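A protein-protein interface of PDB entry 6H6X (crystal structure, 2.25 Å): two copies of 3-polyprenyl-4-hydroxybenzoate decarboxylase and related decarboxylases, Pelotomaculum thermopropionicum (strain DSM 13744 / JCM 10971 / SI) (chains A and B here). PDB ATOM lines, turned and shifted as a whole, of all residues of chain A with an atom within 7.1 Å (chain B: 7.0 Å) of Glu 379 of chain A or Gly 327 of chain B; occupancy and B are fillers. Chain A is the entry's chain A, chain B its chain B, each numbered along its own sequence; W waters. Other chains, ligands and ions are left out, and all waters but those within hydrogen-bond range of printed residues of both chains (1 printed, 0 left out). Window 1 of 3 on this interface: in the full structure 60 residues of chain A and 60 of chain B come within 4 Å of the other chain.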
ATOM      1  N   VAL A 364     -10.640 -37.694 -28.631  1.00  0.00           N
ATOM      2  CA  VAL A 364     -12.017 -37.589 -28.238  1.00  0.00           C
ATOM      3  C   VAL A 364     -13.038 -37.853 -29.351  1.00  0.00           C
ATOM      4  O   VAL A 364     -12.881 -37.346 -30.482  1.00  0.00           O
ATOM      5  CB  VAL A 364     -12.367 -36.411 -27.304  1.00  0.00           C
ATOM      6  CG1 VAL A 364     -11.194 -35.569 -26.803  1.00  0.00           C
ATOM      7  CG2 VAL A 364     -13.619 -35.678 -27.608  1.00  0.00           C
ATOM      8  N   VAL A 366     -17.056 -37.625 -30.529  1.00  0.00           N
ATOM      9  CA  VAL A 366     -18.294 -36.925 -30.259  1.00  0.00           C
ATOM     10  C   VAL A 366     -19.343 -37.267 -31.333  1.00  0.00           C
ATOM     11  O   VAL A 366     -19.017 -37.810 -32.382  1.00  0.00           O
ATOM     12  CB  VAL A 366     -18.131 -35.411 -30.197  1.00  0.00           C
ATOM     13  CG1 VAL A 366     -17.158 -35.057 -29.085  1.00  0.00           C
ATOM     14  CG2 VAL A 366     -17.606 -34.866 -31.527  1.00  0.00           C
ATOM     15  N   ILE A 370     -21.840 -32.101 -33.066  1.00  0.00           N
ATOM     16  CA  ILE A 370     -20.862 -31.249 -32.358  1.00  0.00           C
ATOM     17  C   ILE A 370     -19.937 -30.720 -33.435  1.00  0.00           C
ATOM     18  O   ILE A 370     -19.491 -31.441 -34.329  1.00  0.00           O
ATOM     19  CB  ILE A 370     -20.084 -32.030 -31.278  1.00  0.00           C
ATOM     20  CG1 ILE A 370     -21.023 -32.533 -30.170  1.00  0.00           C
ATOM     21  CG2 ILE A 370     -18.955 -31.180 -30.703  1.00  0.00           C
ATOM     22  CD1 ILE A 370     -21.753 -31.438 -29.387  1.00  0.00           C
ATOM     23  N   ASP A 374     -14.565 -26.422 -33.118  1.00  0.00           N
ATOM     24  CA  ASP A 374     -14.813 -25.454 -32.057  1.00  0.00           C
ATOM     25  C   ASP A 374     -14.447 -26.103 -30.722  1.00  0.00           C
ATOM     26  O   ASP A 374     -15.242 -26.931 -30.193  1.00  0.00           O
ATOM     27  CB  ASP A 374     -16.281 -25.064 -32.065  1.00  0.00           C
ATOM     28  CG  ASP A 374     -16.620 -24.016 -31.041  1.00  0.00           C
ATOM     29  OD1 ASP A 374     -15.819 -23.797 -30.089  1.00  0.00           O
ATOM     30  OD2 ASP A 374     -17.717 -23.422 -31.210  1.00  0.00           O
ATOM     31  N   PRO A 375     -13.275 -25.719 -30.142  1.00  0.00           N
ATOM     32  CA  PRO A 375     -12.821 -26.407 -28.895  1.00  0.00           C
ATOM     33  C   PRO A 375     -13.814 -26.258 -27.738  1.00  0.00           C
ATOM     34  O   PRO A 375     -13.913 -27.144 -26.935  1.00  0.00           O
ATOM     35  CB  PRO A 375     -11.437 -25.763 -28.554  1.00  0.00           C
ATOM     36  CG  PRO A 375     -11.190 -24.723 -29.616  1.00  0.00           C
ATOM     37  CD  PRO A 375     -12.336 -24.672 -30.604  1.00  0.00           C
ATOM     38  N   GLU A 376     -14.534 -25.144 -27.654  1.00  0.00           N
ATOM     39  CA  GLU A 376     -15.463 -24.938 -26.553  1.00  0.00           C
ATOM     40  C   GLU A 376     -16.665 -25.955 -26.585  1.00  0.00           C
ATOM     41  O   GLU A 376     -17.198 -26.380 -25.545  1.00  0.00           O
ATOM     42  CB  GLU A 376     -15.982 -23.502 -26.560  1.00  0.00           C
ATOM     43  CG  GLU A 376     -16.737 -23.145 -25.273  1.00  0.00           C
ATOM     44  CD  GLU A 376     -17.103 -21.640 -25.184  1.00  0.00           C
ATOM     45  OE1 GLU A 376     -16.506 -20.773 -25.895  1.00  0.00           O
ATOM     46  OE2 GLU A 376     -17.994 -21.312 -24.376  1.00  0.00           O
ATOM     47  N   GLU A 377     -17.048 -26.327 -27.794  1.00  0.00           N
ATOM     48  CA  GLU A 377     -18.165 -27.233 -28.010  1.00  0.00           C
ATOM     49  C   GLU A 377     -17.709 -28.674 -27.768  1.00  0.00           C
ATOM     50  O   GLU A 377     -18.409 -29.441 -27.104  1.00  0.00           O
ATOM     51  CB  GLU A 377     -18.756 -27.023 -29.424  1.00  0.00           C
ATOM     52  CG  GLU A 377     -20.273 -26.999 -29.445  1.00  0.00           C
ATOM     53  CD  GLU A 377     -20.828 -26.743 -30.835  1.00  0.00           C
ATOM     54  OE1 GLU A 377     -20.925 -25.559 -31.210  1.00  0.00           O
ATOM     55  OE2 GLU A 377     -21.130 -27.721 -31.552  1.00  0.00           O
ATOM     56  N   VAL A 378     -16.534 -29.039 -28.250  1.00  0.00           N
ATOM     57  CA  VAL A 378     -15.984 -30.325 -27.856  1.00  0.00           C
ATOM     58  C   VAL A 378     -15.803 -30.445 -26.330  1.00  0.00           C
ATOM     59  O   VAL A 378     -16.281 -31.401 -25.751  1.00  0.00           O
ATOM     60  CB  VAL A 378     -14.895 -30.969 -28.768  1.00  0.00           C
ATOM     61  CG1 VAL A 378     -14.576 -30.202 -30.012  1.00  0.00           C
ATOM     62  CG2 VAL A 378     -13.713 -31.603 -28.046  1.00  0.00           C
ATOM     63  N   GLU A 379     -15.314 -29.406 -25.665  1.00  0.00           N
ATOM     64  CA  GLU A 379     -15.169 -29.453 -24.203  1.00  0.00           C
ATOM     65  C   GLU A 379     -16.524 -29.623 -23.523  1.00  0.00           C
ATOM     66  O   GLU A 379     -16.682 -30.350 -22.526  1.00  0.00           O
ATOM     67  CB  GLU A 379     -14.430 -28.190 -23.687  1.00  0.00           C
ATOM     68  CG  GLU A 379     -14.352 -28.120 -22.179  1.00  0.00           C
ATOM     69  CD  GLU A 379     -13.441 -26.998 -21.615  1.00  0.00           C
ATOM     70  OE1 GLU A 379     -13.075 -27.100 -20.420  1.00  0.00           O
ATOM     71  OE2 GLU A 379     -13.108 -26.023 -22.322  1.00  0.00           O
ATOM     72  N   TRP A 380     -17.513 -28.939 -24.068  1.00  0.00           N
ATOM     73  CA  TRP A 380     -18.843 -29.072 -23.546  1.00  0.00           C
ATOM     74  C   TRP A 380     -19.393 -30.496 -23.666  1.00  0.00           C
ATOM     75  O   TRP A 380     -20.002 -30.997 -22.744  1.00  0.00           O
ATOM     76  CB  TRP A 380     -19.738 -28.054 -24.216  1.00  0.00           C
ATOM     77  CG  TRP A 380     -21.091 -28.165 -23.856  1.00  0.00           C
ATOM     78  CD1 TRP A 380     -21.700 -27.673 -22.744  1.00  0.00           C
ATOM     79  CD2 TRP A 380     -22.090 -28.840 -24.599  1.00  0.00           C
ATOM     80  NE1 TRP A 380     -23.040 -28.001 -22.754  1.00  0.00           N
ATOM     81  CE2 TRP A 380     -23.294 -28.736 -23.876  1.00  0.00           C
ATOM     82  CE3 TRP A 380     -22.084 -29.535 -25.815  1.00  0.00           C
ATOM     83  CZ2 TRP A 380     -24.488 -29.247 -24.358  1.00  0.00           C
ATOM     84  CZ3 TRP A 380     -23.280 -30.074 -26.285  1.00  0.00           C
ATOM     85  CH2 TRP A 380     -24.467 -29.911 -25.569  1.00  0.00           C
ATOM     86  N   ALA A 381     -19.167 -31.123 -24.798  1.00  0.00           N
ATOM     87  CA  ALA A 381     -19.510 -32.494 -24.996  1.00  0.00           C
ATOM     88  C   ALA A 381     -18.787 -33.414 -24.009  1.00  0.00           C
ATOM     89  O   ALA A 381     -19.404 -34.317 -23.420  1.00  0.00           O
ATOM     90  CB  ALA A 381     -19.241 -32.893 -26.432  1.00  0.00           C
ATOM     91  N   VAL A 382     -17.494 -33.171 -23.765  1.00  0.00           N
ATOM     92  CA  VAL A 382     -16.773 -33.939 -22.731  1.00  0.00           C
ATOM     93  C   VAL A 382     -17.413 -33.658 -21.349  1.00  0.00           C
ATOM     94  O   VAL A 382     -17.688 -34.582 -20.567  1.00  0.00           O
ATOM     95  CB  VAL A 382     -15.259 -33.623 -22.717  1.00  0.00           C
ATOM     96  CG1 VAL A 382     -14.519 -34.254 -21.512  1.00  0.00           C
ATOM     97  CG2 VAL A 382     -14.614 -34.132 -23.997  1.00  0.00           C
ATOM     98  N   ALA A 383     -17.642 -32.389 -21.031  1.00  0.00           N
ATOM     99  CA  ALA A 383     -18.178 -32.053 -19.723  1.00  0.00           C
ATOM    100  C   ALA A 383     -19.540 -32.736 -19.474  1.00  0.00           C
ATOM    101  O   ALA A 383     -19.793 -33.179 -18.351  1.00  0.00           O
ATOM    102  CB  ALA A 383     -18.336 -30.539 -19.537  1.00  0.00           C
ATOM    103  N   THR A 384     -20.394 -32.838 -20.497  1.00  0.00           N
ATOM    104  CA  THR A 384     -21.757 -33.275 -20.254  1.00  0.00           C
ATOM    105  C   THR A 384     -22.027 -34.726 -20.674  1.00  0.00           C
ATOM    106  O   THR A 384     -22.999 -35.297 -20.244  1.00  0.00           O
ATOM    107  CB  THR A 384     -22.768 -32.262 -20.865  1.00  0.00           C
ATOM    108  OG1 THR A 384     -22.606 -32.217 -22.269  1.00  0.00           O
ATOM    109  CG2 THR A 384     -22.520 -30.812 -20.354  1.00  0.00           C
ATOM    110  N   ARG A 385     -21.171 -35.336 -21.466  1.00  0.00           N
ATOM    111  CA  ARG A 385     -21.399 -36.682 -22.022  1.00  0.00           C
ATOM    112  C   ARG A 385     -20.313 -37.696 -21.742  1.00  0.00           C
ATOM    113  O   ARG A 385     -20.419 -38.821 -22.191  1.00  0.00           O
ATOM    114  CB  ARG A 385     -21.586 -36.610 -23.528  1.00  0.00           C
ATOM    115  CG  ARG A 385     -22.727 -35.699 -23.944  1.00  0.00           C
ATOM    116  CD  ARG A 385     -22.695 -35.352 -25.407  1.00  0.00           C
ATOM    117  NE  ARG A 385     -23.808 -34.461 -25.686  1.00  0.00           N
ATOM    118  CZ  ARG A 385     -24.153 -34.012 -26.886  1.00  0.00           C
ATOM    119  NH1 ARG A 385     -23.443 -34.347 -27.963  1.00  0.00           N
ATOM    120  NH2 ARG A 385     -25.214 -33.220 -27.005  1.00  0.00           N
ATOM    121  N   PRO B 261     -26.322 -25.540 -18.431  1.00  0.00           N
ATOM    122  CA  PRO B 261     -25.473 -26.392 -19.276  1.00  0.00           C
ATOM    123  C   PRO B 261     -25.956 -26.476 -20.751  1.00  0.00           C
ATOM    124  O   PRO B 261     -25.432 -27.324 -21.475  1.00  0.00           O
ATOM    125  CB  PRO B 261     -25.561 -27.779 -18.576  1.00  0.00           C
ATOM    126  CG  PRO B 261     -26.845 -27.763 -17.786  1.00  0.00           C
ATOM    127  CD  PRO B 261     -27.402 -26.354 -17.812  1.00  0.00           C
ATOM    128  N   ARG B 262     -26.918 -25.620 -21.174  1.00  0.00           N
ATOM    129  CA  ARG B 262     -27.468 -25.579 -22.547  1.00  0.00           C
ATOM    130  C   ARG B 262     -28.356 -26.826 -22.851  1.00  0.00           C
ATOM    131  O   ARG B 262     -28.435 -27.296 -23.986  1.00  0.00           O
ATOM    132  CB  ARG B 262     -26.358 -25.330 -23.623  1.00  0.00           C
ATOM    133  CG  ARG B 262     -25.450 -24.098 -23.395  1.00  0.00           C
ATOM    134  CD  ARG B 262     -24.164 -24.106 -24.262  1.00  0.00           C
ATOM    135  NE  ARG B 262     -23.011 -23.469 -23.578  1.00  0.00           N
ATOM    136  CZ  ARG B 262     -21.715 -23.514 -23.959  1.00  0.00           C
ATOM    137  NH1 ARG B 262     -21.323 -24.165 -25.063  1.00  0.00           N
ATOM    138  NH2 ARG B 262     -20.783 -22.885 -23.222  1.00  0.00           N
ATOM    139  N   ARG B 294     -23.123 -15.371 -20.687  1.00  0.00           N
ATOM    140  CA  ARG B 294     -21.891 -15.086 -19.921  1.00  0.00           C
ATOM    141  C   ARG B 294     -22.193 -14.488 -18.589  1.00  0.00           C
ATOM    142  O   ARG B 294     -21.541 -14.842 -17.623  1.00  0.00           O
ATOM    143  CB  ARG B 294     -20.941 -14.146 -20.724  1.00  0.00           C
ATOM    144  CG  ARG B 294     -20.287 -14.815 -21.946  1.00  0.00           C
ATOM    145  CD  ARG B 294     -19.554 -16.093 -21.507  1.00  0.00           C
ATOM    146  NE  ARG B 294     -18.461 -16.576 -22.337  1.00  0.00           N
ATOM    147  CZ  ARG B 294     -18.372 -17.779 -22.936  1.00  0.00           C
ATOM    148  NH1 ARG B 294     -19.352 -18.694 -22.915  1.00  0.00           N
ATOM    149  NH2 ARG B 294     -17.267 -18.053 -23.611  1.00  0.00           N
ATOM    150  N   LEU B 297     -23.326 -17.522 -16.497  1.00  0.00           N
ATOM    151  CA  LEU B 297     -22.185 -18.399 -16.212  1.00  0.00           C
ATOM    152  C   LEU B 297     -21.148 -17.743 -15.281  1.00  0.00           C
ATOM    153  O   LEU B 297     -20.695 -18.380 -14.321  1.00  0.00           O
ATOM    154  CB  LEU B 297     -21.541 -18.847 -17.540  1.00  0.00           C
ATOM    155  CG  LEU B 297     -22.402 -19.743 -18.423  1.00  0.00           C
ATOM    156  CD1 LEU B 297     -21.629 -20.280 -19.587  1.00  0.00           C
ATOM    157  CD2 LEU B 297     -22.929 -20.932 -17.611  1.00  0.00           C
ATOM    158  N   LEU B 324     -12.662 -21.980 -13.699  1.00  0.00           N
ATOM    159  CA  LEU B 324     -13.751 -22.857 -14.160  1.00  0.00           C
ATOM    160  C   LEU B 324     -14.091 -22.432 -15.572  1.00  0.00           C
ATOM    161  O   LEU B 324     -14.611 -21.338 -15.815  1.00  0.00           O
ATOM    162  CB  LEU B 324     -14.929 -22.763 -13.223  1.00  0.00           C
ATOM    163  CG  LEU B 324     -14.633 -23.313 -11.818  1.00  0.00           C
ATOM    164  CD1 LEU B 324     -15.746 -22.967 -10.805  1.00  0.00           C
ATOM    165  CD2 LEU B 324     -14.462 -24.802 -11.849  1.00  0.00           C
ATOM    166  N   THR B 325     -13.794 -23.294 -16.525  1.00  0.00           N
ATOM    167  CA  THR B 325     -13.891 -22.950 -17.955  1.00  0.00           C
ATOM    168  C   THR B 325     -15.341 -22.838 -18.475  1.00  0.00           C
ATOM    169  O   THR B 325     -16.226 -23.516 -17.985  1.00  0.00           O
ATOM    170  CB  THR B 325     -13.201 -23.995 -18.883  1.00  0.00           C
ATOM    171  OG1 THR B 325     -13.896 -25.239 -18.788  1.00  0.00           O
ATOM    172  CG2 THR B 325     -11.756 -24.208 -18.490  1.00  0.00           C
ATOM    173  N   PRO B 326     -15.555 -21.997 -19.475  1.00  0.00           N
ATOM    174  CA  PRO B 326     -16.913 -21.859 -20.033  1.00  0.00           C
ATOM    175  C   PRO B 326     -17.452 -23.114 -20.710  1.00  0.00           C
ATOM    176  O   PRO B 326     -18.633 -23.396 -20.566  1.00  0.00           O
ATOM    177  CB  PRO B 326     -16.793 -20.716 -21.051  1.00  0.00           C
ATOM    178  CG  PRO B 326     -15.340 -20.289 -21.080  1.00  0.00           C
ATOM    179  CD  PRO B 326     -14.644 -20.904 -19.895  1.00  0.00           C
ATOM    180  N   GLY B 327     -16.581 -23.840 -21.405  1.00  0.00           N
ATOM    181  CA  GLY B 327     -16.837 -25.196 -21.875  1.00  0.00           C
ATOM    182  C   GLY B 327     -17.531 -26.104 -20.883  1.00  0.00           C
ATOM    183  O   GLY B 327     -18.476 -26.825 -21.242  1.00  0.00           O
ATOM    184  N   GLY B 328     -17.089 -26.020 -19.625  1.00  0.00           N
ATOM    185  CA  GLY B 328     -17.686 -26.774 -18.523  1.00  0.00           C
ATOM    186  C   GLY B 328     -18.771 -26.093 -17.766  1.00  0.00           C
ATOM    187  O   GLY B 328     -19.106 -26.512 -16.632  1.00  0.00           O
ATOM    188  N   SER B 329     -19.324 -25.041 -18.357  1.00  0.00           N
ATOM    189  CA  SER B 329     -20.408 -24.222 -17.736  1.00  0.00           C
ATOM    190  C   SER B 329     -20.008 -23.511 -16.447  1.00  0.00           C
ATOM    191  O   SER B 329     -20.840 -23.278 -15.556  1.00  0.00           O
ATOM    192  CB  SER B 329     -21.717 -25.039 -17.570  1.00  0.00           C
ATOM    193  OG  SER B 329     -21.969 -25.667 -18.805  1.00  0.00           O
ATOM    194  N   CYS B 330     -18.731 -23.105 -16.393  1.00  0.00           N
ATOM    195  CA  CYS B 330     -18.127 -22.509 -15.201  1.00  0.00           C
ATOM    196  C   CYS B 330     -18.521 -23.242 -13.959  1.00  0.00           C
ATOM    197  O   CYS B 330     -18.956 -22.677 -12.975  1.00  0.00           O
ATOM    198  CB  CYS B 330     -18.406 -21.004 -15.122  1.00  0.00           C
ATOM    199  SG  CYS B 330     -17.862 -20.131 -16.622  1.00  0.00           S
ATOM    200  N   TYR B 332     -18.077 -27.488 -14.186  1.00  0.00           N
ATOM    201  CA  TYR B 332     -17.696 -28.902 -14.251  1.00  0.00           C
ATOM    202  C   TYR B 332     -16.204 -29.109 -14.427  1.00  0.00           C
ATOM    203  O   TYR B 332     -15.725 -30.166 -14.008  1.00  0.00           O
ATOM    204  CB  TYR B 332     -18.458 -29.599 -15.392  1.00  0.00           C
ATOM    205  CG  TYR B 332     -19.946 -29.628 -15.199  1.00  0.00           C
ATOM    206  CD1 TYR B 332     -20.491 -30.071 -13.985  1.00  0.00           C
ATOM    207  CD2 TYR B 332     -20.821 -29.185 -16.209  1.00  0.00           C
ATOM    208  CE1 TYR B 332     -21.856 -30.051 -13.775  1.00  0.00           C
ATOM    209  CE2 TYR B 332     -22.185 -29.190 -16.015  1.00  0.00           C
ATOM    210  CZ  TYR B 332     -22.714 -29.624 -14.802  1.00  0.00           C
ATOM    211  OH  TYR B 332     -24.075 -29.625 -14.579  1.00  0.00           O
ATOM    212  N   HIS B 333     -15.543 -28.172 -15.137  1.00  0.00           N
ATOM    213  CA  HIS B 333     -14.174 -28.275 -15.550  1.00  0.00           C
ATOM    214  C   HIS B 333     -13.310 -27.193 -14.868  1.00  0.00           C
ATOM    215  O   HIS B 333     -13.572 -25.994 -15.017  1.00  0.00           O
ATOM    216  CB  HIS B 333     -14.070 -28.109 -17.072  1.00  0.00           C
ATOM    217  CG  HIS B 333     -14.454 -29.341 -17.840  1.00  0.00           C
ATOM    218  ND1 HIS B 333     -14.170 -29.513 -19.173  1.00  0.00           N
ATOM    219  CD2 HIS B 333     -15.099 -30.461 -17.454  1.00  0.00           C
ATOM    220  CE1 HIS B 333     -14.604 -30.701 -19.568  1.00  0.00           C
ATOM    221  NE2 HIS B 333     -15.138 -31.313 -18.528  1.00  0.00           N
ATOM    222  N   ALA B 334     -12.249 -27.619 -14.193  1.00  0.00           N
ATOM    223  CA  ALA B 334     -11.314 -26.717 -13.506  1.00  0.00           C
ATOM    224  C   ALA B 334      -9.898 -26.813 -14.015  1.00  0.00           C
ATOM    225  O   ALA B 334      -9.428 -27.879 -14.356  1.00  0.00           O
ATOM    226  CB  ALA B 334     -11.373 -26.924 -12.015  1.00  0.00           C
ATOM    227  N   VAL B 335      -9.280 -25.655 -14.213  1.00  0.00           N
ATOM    228  CA  VAL B 335      -7.871 -25.550 -14.538  1.00  0.00           C
ATOM    229  C   VAL B 335      -7.207 -24.873 -13.324  1.00  0.00           C
ATOM    230  O   VAL B 335      -7.658 -23.812 -12.888  1.00  0.00           O
ATOM    231  CB  VAL B 335      -7.603 -24.809 -15.857  1.00  0.00           C
ATOM    232  CG1 VAL B 335      -6.119 -24.797 -16.169  1.00  0.00           C
ATOM    233  CG2 VAL B 335      -8.352 -25.477 -17.023  1.00  0.00           C
ATOM    234  N   HIS B 362     -13.760 -32.636 -13.692  1.00  0.00           N
ATOM    235  CA  HIS B 362     -12.553 -32.751 -14.494  1.00  0.00           C
ATOM    236  C   HIS B 362     -11.638 -31.597 -14.075  1.00  0.00           C
ATOM    237  O   HIS B 362     -12.054 -30.416 -14.078  1.00  0.00           O
ATOM    238  CB  HIS B 362     -13.011 -32.615 -15.927  1.00  0.00           C
ATOM    239  CG  HIS B 362     -11.945 -32.748 -16.954  1.00  0.00           C
ATOM    240  ND1 HIS B 362     -11.127 -31.688 -17.320  1.00  0.00           N
ATOM    241  CD2 HIS B 362     -11.617 -33.782 -17.774  1.00  0.00           C
ATOM    242  CE1 HIS B 362     -10.325 -32.082 -18.303  1.00  0.00           C
ATOM    243  NE2 HIS B 362     -10.617 -33.338 -18.614  1.00  0.00           N
ATOM    244  N   PRO B 375      -7.670 -21.677 -23.606  1.00  0.00           N
ATOM    245  CA  PRO B 375      -7.858 -23.154 -23.748  1.00  0.00           C
ATOM    246  C   PRO B 375      -6.829 -23.793 -24.643  1.00  0.00           C
ATOM    247  O   PRO B 375      -6.486 -24.942 -24.411  1.00  0.00           O
ATOM    248  CB  PRO B 375      -9.306 -23.328 -24.318  1.00  0.00           C
ATOM    249  CG  PRO B 375      -9.865 -21.911 -24.505  1.00  0.00           C
ATOM    250  CD  PRO B 375      -8.837 -20.881 -24.082  1.00  0.00           C
HETATM  251  O   HOH W   1     -13.782 -23.227 -22.330  1.00  0.00           O
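Hydrophobic or aromatic side chains of chain B within 4 Å of the printed part of chain A: Pro 326 and His 333.
The backbone carbonyl oxygen (O) of Pro 326 of chain B sits at hydrogen-bond distance from the guanidinium group (NH2) of Arg 262 of chain B (3.5 Å). N of Gly 328 of chain B is in hydrogen-bond range of OG1 of Thr 325 of chain B. N of Cys 330 of chain B is in hydrogen-bond range of O of Thr 325 of chain B (3.0 Å). N of Thr 325 of chain B lies within hydrogen-bond range of O of His 333 of chain B, 3.1 Å away. The side-chain carboxylate (OD1) of Asp 374 of chain A lies within hydrogen-bond range of the backbone NH (N) of Glu 376 of chain A, at 3.1 Å. OG1 of Thr 384 of chain A is in hydrogen-bond range of O of Trp 380 of chain A, at 2.9 Å.
Water W1 bridges OE2 of Glu 379 of chain A (2.9 Å) and N of Gly 327 of chain B (3.0 Å).
The backbone carbonyl oxygen of Pro 261 of chain B is in hydrogen-bond range of the indole nitrogen of Trp 380 of chain A, at 2.8 Å. The guanidinium group (NH2) of Arg 262 of chain B lies within salt-bridge range of the side-chain carboxylate (OE2) of Glu 376 of chain A. NH1 of Arg 294 of chain B lies within salt-bridge range of OE2 of Glu 376 of chain A (3.3 Å). OG1 of Thr 325 of chain B is in hydrogen-bond range of OE1 of Glu 379 of chain A (2.6 Å). ND1 of His 333 of chain B lies within hydrogen-bond range of OE1 of Glu 379 of chain A (2.9 Å).
Printed residues of chain B within 4 Å of Glu 376 of chain A: Arg 262 (3.4 Å), Arg 294 (3.3 Å), Pro 326 (3.6 Å) and Gly 327 (3.9 Å). Glu 377 of chain A touches none of the printed residues of chain B. Glu 379 of chain A touches three residues of chain B. Arg 385 of chain A touches none of the printed residues of chain B. Of the printed residues of chain A, Pro 261 of chain B touches Trp 380. Of the printed residues of chain A, Thr 325 of chain B touches Glu 379. Of chain A, only Glu 376 (3.9 Å), Glu 379 (3.8 Å) and Trp 380 (3.2 Å) come within 4 Å of Gly 327 of chain B. Printed residues of chain A within 4 Å of Gly 328 of chain B: Ala 383 (3.95 Å). The nearest printed residue of chain A that does not touch Pro 261 of chain B is Thr 384 of chain A (4.6 Å).
Among the printed residues, merely in contact across the chains: Trp 380 of chain A with Gly 327 of chain B, Ala 383 of chain A with His 333 of chain B, Glu 376 of chain A with Pro 326 of chain B, Glu 379 of chain A with Gly 327 of chain B, Glu 376 of chain A with Gly 327 of chain B and Ala 383 of chain A with Gly 328 of chain B.
Position printed for both chains: 375.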
